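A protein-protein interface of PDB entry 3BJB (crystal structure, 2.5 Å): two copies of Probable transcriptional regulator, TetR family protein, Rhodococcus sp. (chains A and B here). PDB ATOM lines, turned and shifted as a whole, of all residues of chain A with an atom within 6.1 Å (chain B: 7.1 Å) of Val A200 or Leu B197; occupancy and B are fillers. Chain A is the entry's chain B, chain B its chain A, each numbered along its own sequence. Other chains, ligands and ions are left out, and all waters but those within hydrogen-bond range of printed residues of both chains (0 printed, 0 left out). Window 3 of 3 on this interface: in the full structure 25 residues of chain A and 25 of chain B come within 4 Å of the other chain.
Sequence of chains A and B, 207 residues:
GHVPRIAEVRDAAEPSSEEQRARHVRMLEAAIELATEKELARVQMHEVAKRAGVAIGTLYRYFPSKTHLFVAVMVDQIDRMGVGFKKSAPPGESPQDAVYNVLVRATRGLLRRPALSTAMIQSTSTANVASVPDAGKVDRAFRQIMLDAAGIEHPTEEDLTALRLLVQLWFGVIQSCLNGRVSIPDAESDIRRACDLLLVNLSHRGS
Of the printed residues of chain B, Leu A197 touches Leu B197 (3.9 Å) and Leu B198 (3.6 Å). Printed residues of chain B within 4 Å of Leu A198: Leu B197 (3.6 Å) and Leu B198 (3.6 Å). Of chain A, only Leu A197 (3.9 Å), Leu A198 (3.6 Å) and Val A200 (3.9 Å) come within 4 Å of Leu B197. The nearest residue of chain A that does not touch Leu B197 is Asn A201 (4.2 Å).
Printed residues of chain A that touch a printed residue of chain B: Glu A158, Leu A165, Leu A197, Leu A198 and Val A200. Hydrophobic or aromatic side chains of chain A within 4 Å of the printed part of chain B: Leu A165, Leu A197, Leu A198 and Val A200. Among the printed residues, 8 pairs touch across the chains. Among the printed residues, Asp or Glu carboxylates within 4 Å of a Lys or Arg side-chain nitrogen of the other chain: Glu A158 with Arg B193.
OE2 of Glu A158 lies within salt-bridge range of NH1 of Arg B193 (3.7 Å).
The side-chain carboxylate (OE2) of Glu A158 sits at hydrogen-bond distance from the side-chain amide nitrogen (ND2) of Asn A201 (3.3 Å).
Leu A165 touches Arg B193. Ala B194 touches Leu A165. O of Leu A197 touches O of Leu B197, 3.9 Å away. O of Leu B198 touches CD1 of Leu A197 (3.6 Å). Leu A198 touches Leu B197. CD2 of Leu B198 touches CG of Leu A198, at 3.6 Å. Leu B197 touches Val A200 (CD2 to CG2, 3.9 Å).
Leu B197 touches its own counterpart, Leu A197. Leu A197 touches Leu B198, and with the chains exchanged Leu A198 touches Leu B197. Leu A198 touches its own counterpart, Leu B198. Val A200 touches Leu B197, but with the chains exchanged Leu A197 does not touch Val B200 (4.4 Å). Positions printed for both chains: 195, 196, 197, 198, 199, 200 and 201.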
ATOM      1  N   GLN A  96      13.978  11.883 -21.995  1.00  0.00           N
ATOM      2  CA  GLN A  96      14.320  10.650 -22.671  1.00  0.00           C
ATOM      3  C   GLN A  96      15.842  10.525 -22.888  1.00  0.00           C
ATOM      4  O   GLN A  96      16.432   9.458 -22.741  1.00  0.00           O
ATOM      5  CB  GLN A  96      13.448  10.373 -23.929  1.00  0.00           C
ATOM      6  CG  GLN A  96      12.927  11.525 -24.769  1.00  0.00           C
ATOM      7  CD  GLN A  96      11.925  12.421 -24.047  1.00  0.00           C
ATOM      8  OE1 GLN A  96      12.269  13.525 -23.625  1.00  0.00           O
ATOM      9  NE2 GLN A  96      10.689  11.962 -23.919  1.00  0.00           N
ATOM     10  N   GLU A 158       1.285   5.762 -17.031  1.00  0.00           N
ATOM     11  CA  GLU A 158       1.775   5.641 -18.391  1.00  0.00           C
ATOM     12  C   GLU A 158       3.316   5.695 -18.452  1.00  0.00           C
ATOM     13  O   GLU A 158       3.925   4.877 -19.147  1.00  0.00           O
ATOM     14  CB  GLU A 158       1.177   6.741 -19.274  1.00  0.00           C
ATOM     15  CG  GLU A 158       0.835   6.264 -20.675  1.00  0.00           C
ATOM     16  CD  GLU A 158       1.487   7.102 -21.763  1.00  0.00           C
ATOM     17  OE1 GLU A 158       1.046   8.271 -21.973  1.00  0.00           O
ATOM     18  OE2 GLU A 158       2.441   6.566 -22.414  1.00  0.00           O
ATOM     19  N   ALA A 162       5.841   2.749 -19.375  1.00  0.00           N
ATOM     20  CA  ALA A 162       6.918   2.996 -20.366  1.00  0.00           C
ATOM     21  C   ALA A 162       8.293   2.574 -19.863  1.00  0.00           C
ATOM     22  O   ALA A 162       9.025   1.861 -20.542  1.00  0.00           O
ATOM     23  CB  ALA A 162       6.927   4.452 -20.817  1.00  0.00           C
ATOM     24  N   LEU A 165       8.558  -1.280 -19.508  1.00  0.00           N
ATOM     25  CA  LEU A 165       8.903  -1.738 -20.860  1.00  0.00           C
ATOM     26  C   LEU A 165      10.383  -1.479 -21.269  1.00  0.00           C
ATOM     27  O   LEU A 165      11.011  -2.322 -21.908  1.00  0.00           O
ATOM     28  CB  LEU A 165       7.944  -1.128 -21.883  1.00  0.00           C
ATOM     29  CG  LEU A 165       6.453  -1.505 -21.776  1.00  0.00           C
ATOM     30  CD1 LEU A 165       5.629  -0.766 -22.841  1.00  0.00           C
ATOM     31  CD2 LEU A 165       6.222  -2.976 -21.917  1.00  0.00           C
ATOM     32  N   CYS A 195      14.579   4.106 -26.245  1.00  0.00           N
ATOM     33  CA  CYS A 195      14.248   5.336 -25.508  1.00  0.00           C
ATOM     34  C   CYS A 195      13.319   6.295 -26.257  1.00  0.00           C
ATOM     35  O   CYS A 195      12.373   6.825 -25.682  1.00  0.00           O
ATOM     36  CB  CYS A 195      15.514   6.065 -25.087  1.00  0.00           C
ATOM     37  SG  CYS A 195      16.302   5.203 -23.770  1.00  0.00           S
ATOM     38  N   ASP A 196      13.604   6.508 -27.535  1.00  0.00           N
ATOM     39  CA  ASP A 196      12.877   7.487 -28.342  1.00  0.00           C
ATOM     40  C   ASP A 196      11.483   6.974 -28.622  1.00  0.00           C
ATOM     41  O   ASP A 196      10.486   7.737 -28.610  1.00  0.00           O
ATOM     42  CB  ASP A 196      13.570   7.702 -29.685  1.00  0.00           C
ATOM     43  CG  ASP A 196      14.904   8.438 -29.563  1.00  0.00           C
ATOM     44  OD1 ASP A 196      15.319   8.816 -28.438  1.00  0.00           O
ATOM     45  OD2 ASP A 196      15.555   8.633 -30.614  1.00  0.00           O
ATOM     46  N   LEU A 197      11.414   5.673 -28.888  1.00  0.00           N
ATOM     47  CA  LEU A 197      10.138   5.074 -29.174  1.00  0.00           C
ATOM     48  C   LEU A 197       9.304   4.967 -27.900  1.00  0.00           C
ATOM     49  O   LEU A 197       8.169   5.509 -27.847  1.00  0.00           O
ATOM     50  CB  LEU A 197      10.312   3.746 -29.915  1.00  0.00           C
ATOM     51  CG  LEU A 197      10.794   4.032 -31.340  1.00  0.00           C
ATOM     52  CD1 LEU A 197      11.079   2.768 -32.103  1.00  0.00           C
ATOM     53  CD2 LEU A 197       9.819   4.949 -32.151  1.00  0.00           C
ATOM     54  N   LEU A 198       9.869   4.324 -26.873  1.00  0.00           N
ATOM     55  CA  LEU A 198       9.117   4.012 -25.656  1.00  0.00           C
ATOM     56  C   LEU A 198       8.740   5.208 -24.825  1.00  0.00           C
ATOM     57  O   LEU A 198       7.674   5.201 -24.222  1.00  0.00           O
ATOM     58  CB  LEU A 198       9.818   2.990 -24.764  1.00  0.00           C
ATOM     59  CG  LEU A 198       9.780   1.545 -25.291  1.00  0.00           C
ATOM     60  CD1 LEU A 198      10.879   0.651 -24.760  1.00  0.00           C
ATOM     61  CD2 LEU A 198       8.433   0.915 -25.022  1.00  0.00           C
ATOM     62  N   LEU A 199       9.591   6.235 -24.806  1.00  0.00           N
ATOM     63  CA  LEU A 199       9.386   7.374 -23.891  1.00  0.00           C
ATOM     64  C   LEU A 199       8.869   8.676 -24.504  1.00  0.00           C
ATOM     65  O   LEU A 199       9.079   9.746 -23.928  1.00  0.00           O
ATOM     66  CB  LEU A 199      10.666   7.659 -23.092  1.00  0.00           C
ATOM     67  CG  LEU A 199      11.369   6.501 -22.391  1.00  0.00           C
ATOM     68  CD1 LEU A 199      12.701   7.012 -21.860  1.00  0.00           C
ATOM     69  CD2 LEU A 199      10.496   5.915 -21.278  1.00  0.00           C
ATOM     70  N   VAL A 200       8.173   8.588 -25.638  1.00  0.00           N
ATOM     71  CA  VAL A 200       7.551   9.776 -26.260  1.00  0.00           C
ATOM     72  C   VAL A 200       6.799  10.651 -25.280  1.00  0.00           C
ATOM     73  O   VAL A 200       6.922  11.862 -25.348  1.00  0.00           O
ATOM     74  CB  VAL A 200       6.558   9.441 -27.397  1.00  0.00           C
ATOM     75  CG1 VAL A 200       7.226   9.579 -28.738  1.00  0.00           C
ATOM     76  CG2 VAL A 200       5.906   8.058 -27.200  1.00  0.00           C
ATOM     77  N   ASN A 201       6.044  10.041 -24.366  1.00  0.00           N
ATOM     78  CA  ASN A 201       5.091  10.778 -23.513  1.00  0.00           C
ATOM     79  C   ASN A 201       5.579  11.124 -22.099  1.00  0.00           C
ATOM     80  O   ASN A 201       4.782  11.399 -21.202  1.00  0.00           O
ATOM     81  CB  ASN A 201       3.762  10.015 -23.464  1.00  0.00           C
ATOM     82  CG  ASN A 201       3.244   9.678 -24.856  1.00  0.00           C
ATOM     83  OD1 ASN A 201       2.973  10.575 -25.669  1.00  0.00           O
ATOM     84  ND2 ASN A 201       3.116   8.383 -25.144  1.00  0.00           N
ATOM     85  N   LEU A 202       6.898  11.116 -21.923  1.00  0.00           N
ATOM     86  CA  LEU A 202       7.518  11.384 -20.632  1.00  0.00           C
ATOM     87  C   LEU A 202       7.498  12.875 -20.196  1.00  0.00           C
ATOM     88  O   LEU A 202       8.356  13.673 -20.606  1.00  0.00           O
ATOM     89  CB  LEU A 202       8.931  10.814 -20.630  1.00  0.00           C
ATOM     90  CG  LEU A 202       9.239  10.052 -19.349  1.00  0.00           C
ATOM     91  CD1 LEU A 202       8.574   8.697 -19.381  1.00  0.00           C
ATOM     92  CD2 LEU A 202      10.713   9.898 -19.186  1.00  0.00           C
ATOM     93  N   ILE B 191       2.603  -6.094 -23.976  1.00  0.00           N
ATOM     94  CA  ILE B 191       2.977  -6.332 -25.361  1.00  0.00           C
ATOM     95  C   ILE B 191       2.101  -5.432 -26.251  1.00  0.00           C
ATOM     96  O   ILE B 191       2.546  -4.919 -27.285  1.00  0.00           O
ATOM     97  CB  ILE B 191       3.011  -7.861 -25.757  1.00  0.00           C
ATOM     98  CG1 ILE B 191       1.839  -8.253 -26.634  1.00  0.00           C
ATOM     99  CG2 ILE B 191       3.120  -8.777 -24.549  1.00  0.00           C
ATOM    100  CD1 ILE B 191       2.164  -8.211 -28.132  1.00  0.00           C
ATOM    101  N   ARG B 192       0.867  -5.197 -25.806  1.00  0.00           N
ATOM    102  CA  ARG B 192      -0.021  -4.271 -26.500  1.00  0.00           C
ATOM    103  C   ARG B 192       0.659  -2.882 -26.573  1.00  0.00           C
ATOM    104  O   ARG B 192       0.907  -2.368 -27.672  1.00  0.00           O
ATOM    105  CB  ARG B 192      -1.424  -4.240 -25.853  1.00  0.00           C
ATOM    106  CG  ARG B 192      -2.468  -3.254 -26.509  1.00  0.00           C
ATOM    107  CD  ARG B 192      -3.127  -3.820 -27.774  1.00  0.00           C
ATOM    108  NE  ARG B 192      -4.565  -4.133 -27.643  1.00  0.00           N
ATOM    109  CZ  ARG B 192      -5.111  -5.041 -26.822  1.00  0.00           C
ATOM    110  NH1 ARG B 192      -6.425  -5.223 -26.829  1.00  0.00           N
ATOM    111  NH2 ARG B 192      -4.369  -5.754 -25.975  1.00  0.00           N
ATOM    112  N   ARG B 193       1.019  -2.317 -25.414  1.00  0.00           N
ATOM    113  CA  ARG B 193       1.697  -1.012 -25.364  1.00  0.00           C
ATOM    114  C   ARG B 193       2.939  -1.088 -26.225  1.00  0.00           C
ATOM    115  O   ARG B 193       3.052  -0.368 -27.212  1.00  0.00           O
ATOM    116  CB  ARG B 193       2.068  -0.597 -23.930  1.00  0.00           C
ATOM    117  CG  ARG B 193       0.906  -0.392 -22.930  1.00  0.00           C
ATOM    118  CD  ARG B 193       0.097   0.905 -23.163  1.00  0.00           C
ATOM    119  NE  ARG B 193       0.934   2.008 -23.635  1.00  0.00           N
ATOM    120  CZ  ARG B 193       0.491   3.034 -24.360  1.00  0.00           C
ATOM    121  NH1 ARG B 193       1.339   3.981 -24.748  1.00  0.00           N
ATOM    122  NH2 ARG B 193      -0.787   3.121 -24.709  1.00  0.00           N
ATOM    123  N   ALA B 194       3.841  -1.998 -25.859  1.00  0.00           N
ATOM    124  CA  ALA B 194       5.084  -2.232 -26.585  1.00  0.00           C
ATOM    125  C   ALA B 194       4.884  -2.155 -28.102  1.00  0.00           C
ATOM    126  O   ALA B 194       5.602  -1.419 -28.793  1.00  0.00           O
ATOM    127  CB  ALA B 194       5.641  -3.560 -26.204  1.00  0.00           C
ATOM    128  N   CYS B 195       3.892  -2.901 -28.600  1.00  0.00           N
ATOM    129  CA  CYS B 195       3.542  -2.895 -30.015  1.00  0.00           C
ATOM    130  C   CYS B 195       3.214  -1.502 -30.482  1.00  0.00           C
ATOM    131  O   CYS B 195       3.908  -0.946 -31.332  1.00  0.00           O
ATOM    132  CB  CYS B 195       2.350  -3.811 -30.293  1.00  0.00           C
ATOM    133  SG  CYS B 195       2.784  -5.556 -30.418  1.00  0.00           S
ATOM    134  N   ASP B 196       2.163  -0.929 -29.912  1.00  0.00           N
ATOM    135  CA  ASP B 196       1.741   0.424 -30.253  1.00  0.00           C
ATOM    136  C   ASP B 196       2.861   1.463 -30.152  1.00  0.00           C
ATOM    137  O   ASP B 196       2.999   2.316 -31.029  1.00  0.00           O
ATOM    138  CB  ASP B 196       0.539   0.830 -29.400  1.00  0.00           C
ATOM    139  CG  ASP B 196      -0.742   0.156 -29.858  1.00  0.00           C
ATOM    140  OD1 ASP B 196      -1.037  -0.971 -29.400  1.00  0.00           O
ATOM    141  OD2 ASP B 196      -1.463   0.758 -30.685  1.00  0.00           O
ATOM    142  N   LEU B 197       3.660   1.391 -29.092  1.00  0.00           N
ATOM    143  CA  LEU B 197       4.675   2.403 -28.859  1.00  0.00           C
ATOM    144  C   LEU B 197       5.859   2.216 -29.788  1.00  0.00           C
ATOM    145  O   LEU B 197       6.324   3.182 -30.385  1.00  0.00           O
ATOM    146  CB  LEU B 197       5.140   2.401 -27.407  1.00  0.00           C
ATOM    147  CG  LEU B 197       4.293   3.089 -26.348  1.00  0.00           C
ATOM    148  CD1 LEU B 197       4.959   2.890 -24.994  1.00  0.00           C
ATOM    149  CD2 LEU B 197       4.142   4.576 -26.673  1.00  0.00           C
ATOM    150  N   LEU B 198       6.341   0.974 -29.912  1.00  0.00           N
ATOM    151  CA  LEU B 198       7.494   0.673 -30.764  1.00  0.00           C
ATOM    152  C   LEU B 198       7.183   0.789 -32.250  1.00  0.00           C
ATOM    153  O   LEU B 198       8.068   1.102 -33.040  1.00  0.00           O
ATOM    154  CB  LEU B 198       8.081  -0.700 -30.450  1.00  0.00           C
ATOM    155  CG  LEU B 198       8.694  -0.895 -29.053  1.00  0.00           C
ATOM    156  CD1 LEU B 198       9.491  -2.190 -28.954  1.00  0.00           C
ATOM    157  CD2 LEU B 198       9.556   0.265 -28.649  1.00  0.00           C
ATOM    158  N   LEU B 199       5.925   0.571 -32.624  1.00  0.00           N
ATOM    159  CA  LEU B 199       5.568   0.502 -34.036  1.00  0.00           C
ATOM    160  C   LEU B 199       4.685   1.657 -34.540  1.00  0.00           C
ATOM    161  O   LEU B 199       4.002   1.501 -35.556  1.00  0.00           O
ATOM    162  CB  LEU B 199       4.900  -0.846 -34.343  1.00  0.00           C
ATOM    163  CG  LEU B 199       5.519  -2.139 -33.805  1.00  0.00           C
ATOM    164  CD1 LEU B 199       4.474  -3.219 -33.685  1.00  0.00           C
ATOM    165  CD2 LEU B 199       6.647  -2.617 -34.668  1.00  0.00           C
ATOM    166  N   VAL B 200       4.701   2.808 -33.862  1.00  0.00           N
ATOM    167  CA  VAL B 200       3.882   3.948 -34.301  1.00  0.00           C
ATOM    168  C   VAL B 200       4.014   4.210 -35.802  1.00  0.00           C
ATOM    169  O   VAL B 200       3.025   4.542 -36.476  1.00  0.00           O
ATOM    170  CB  VAL B 200       4.136   5.284 -33.523  1.00  0.00           C
ATOM    171  CG1 VAL B 200       3.027   5.540 -32.491  1.00  0.00           C
ATOM    172  CG2 VAL B 200       5.528   5.323 -32.898  1.00  0.00           C
ATOM    173  N   ASN B 201       5.226   4.042 -36.334  1.00  0.00           N
ATOM    174  CA  ASN B 201       5.437   4.314 -37.756  1.00  0.00           C
ATOM    175  C   ASN B 201       6.137   3.224 -38.550  1.00  0.00           C
ATOM    176  O   ASN B 201       7.120   3.467 -39.244  1.00  0.00           O
ATOM    177  CB  ASN B 201       6.019   5.728 -38.010  1.00  0.00           C
ATOM    178  CG  ASN B 201       7.323   5.999 -37.254  1.00  0.00           C
ATOM    179  OD1 ASN B 201       8.057   6.923 -37.613  1.00  0.00           O
ATOM    180  ND2 ASN B 201       7.605   5.217 -36.207  1.00  0.00           N
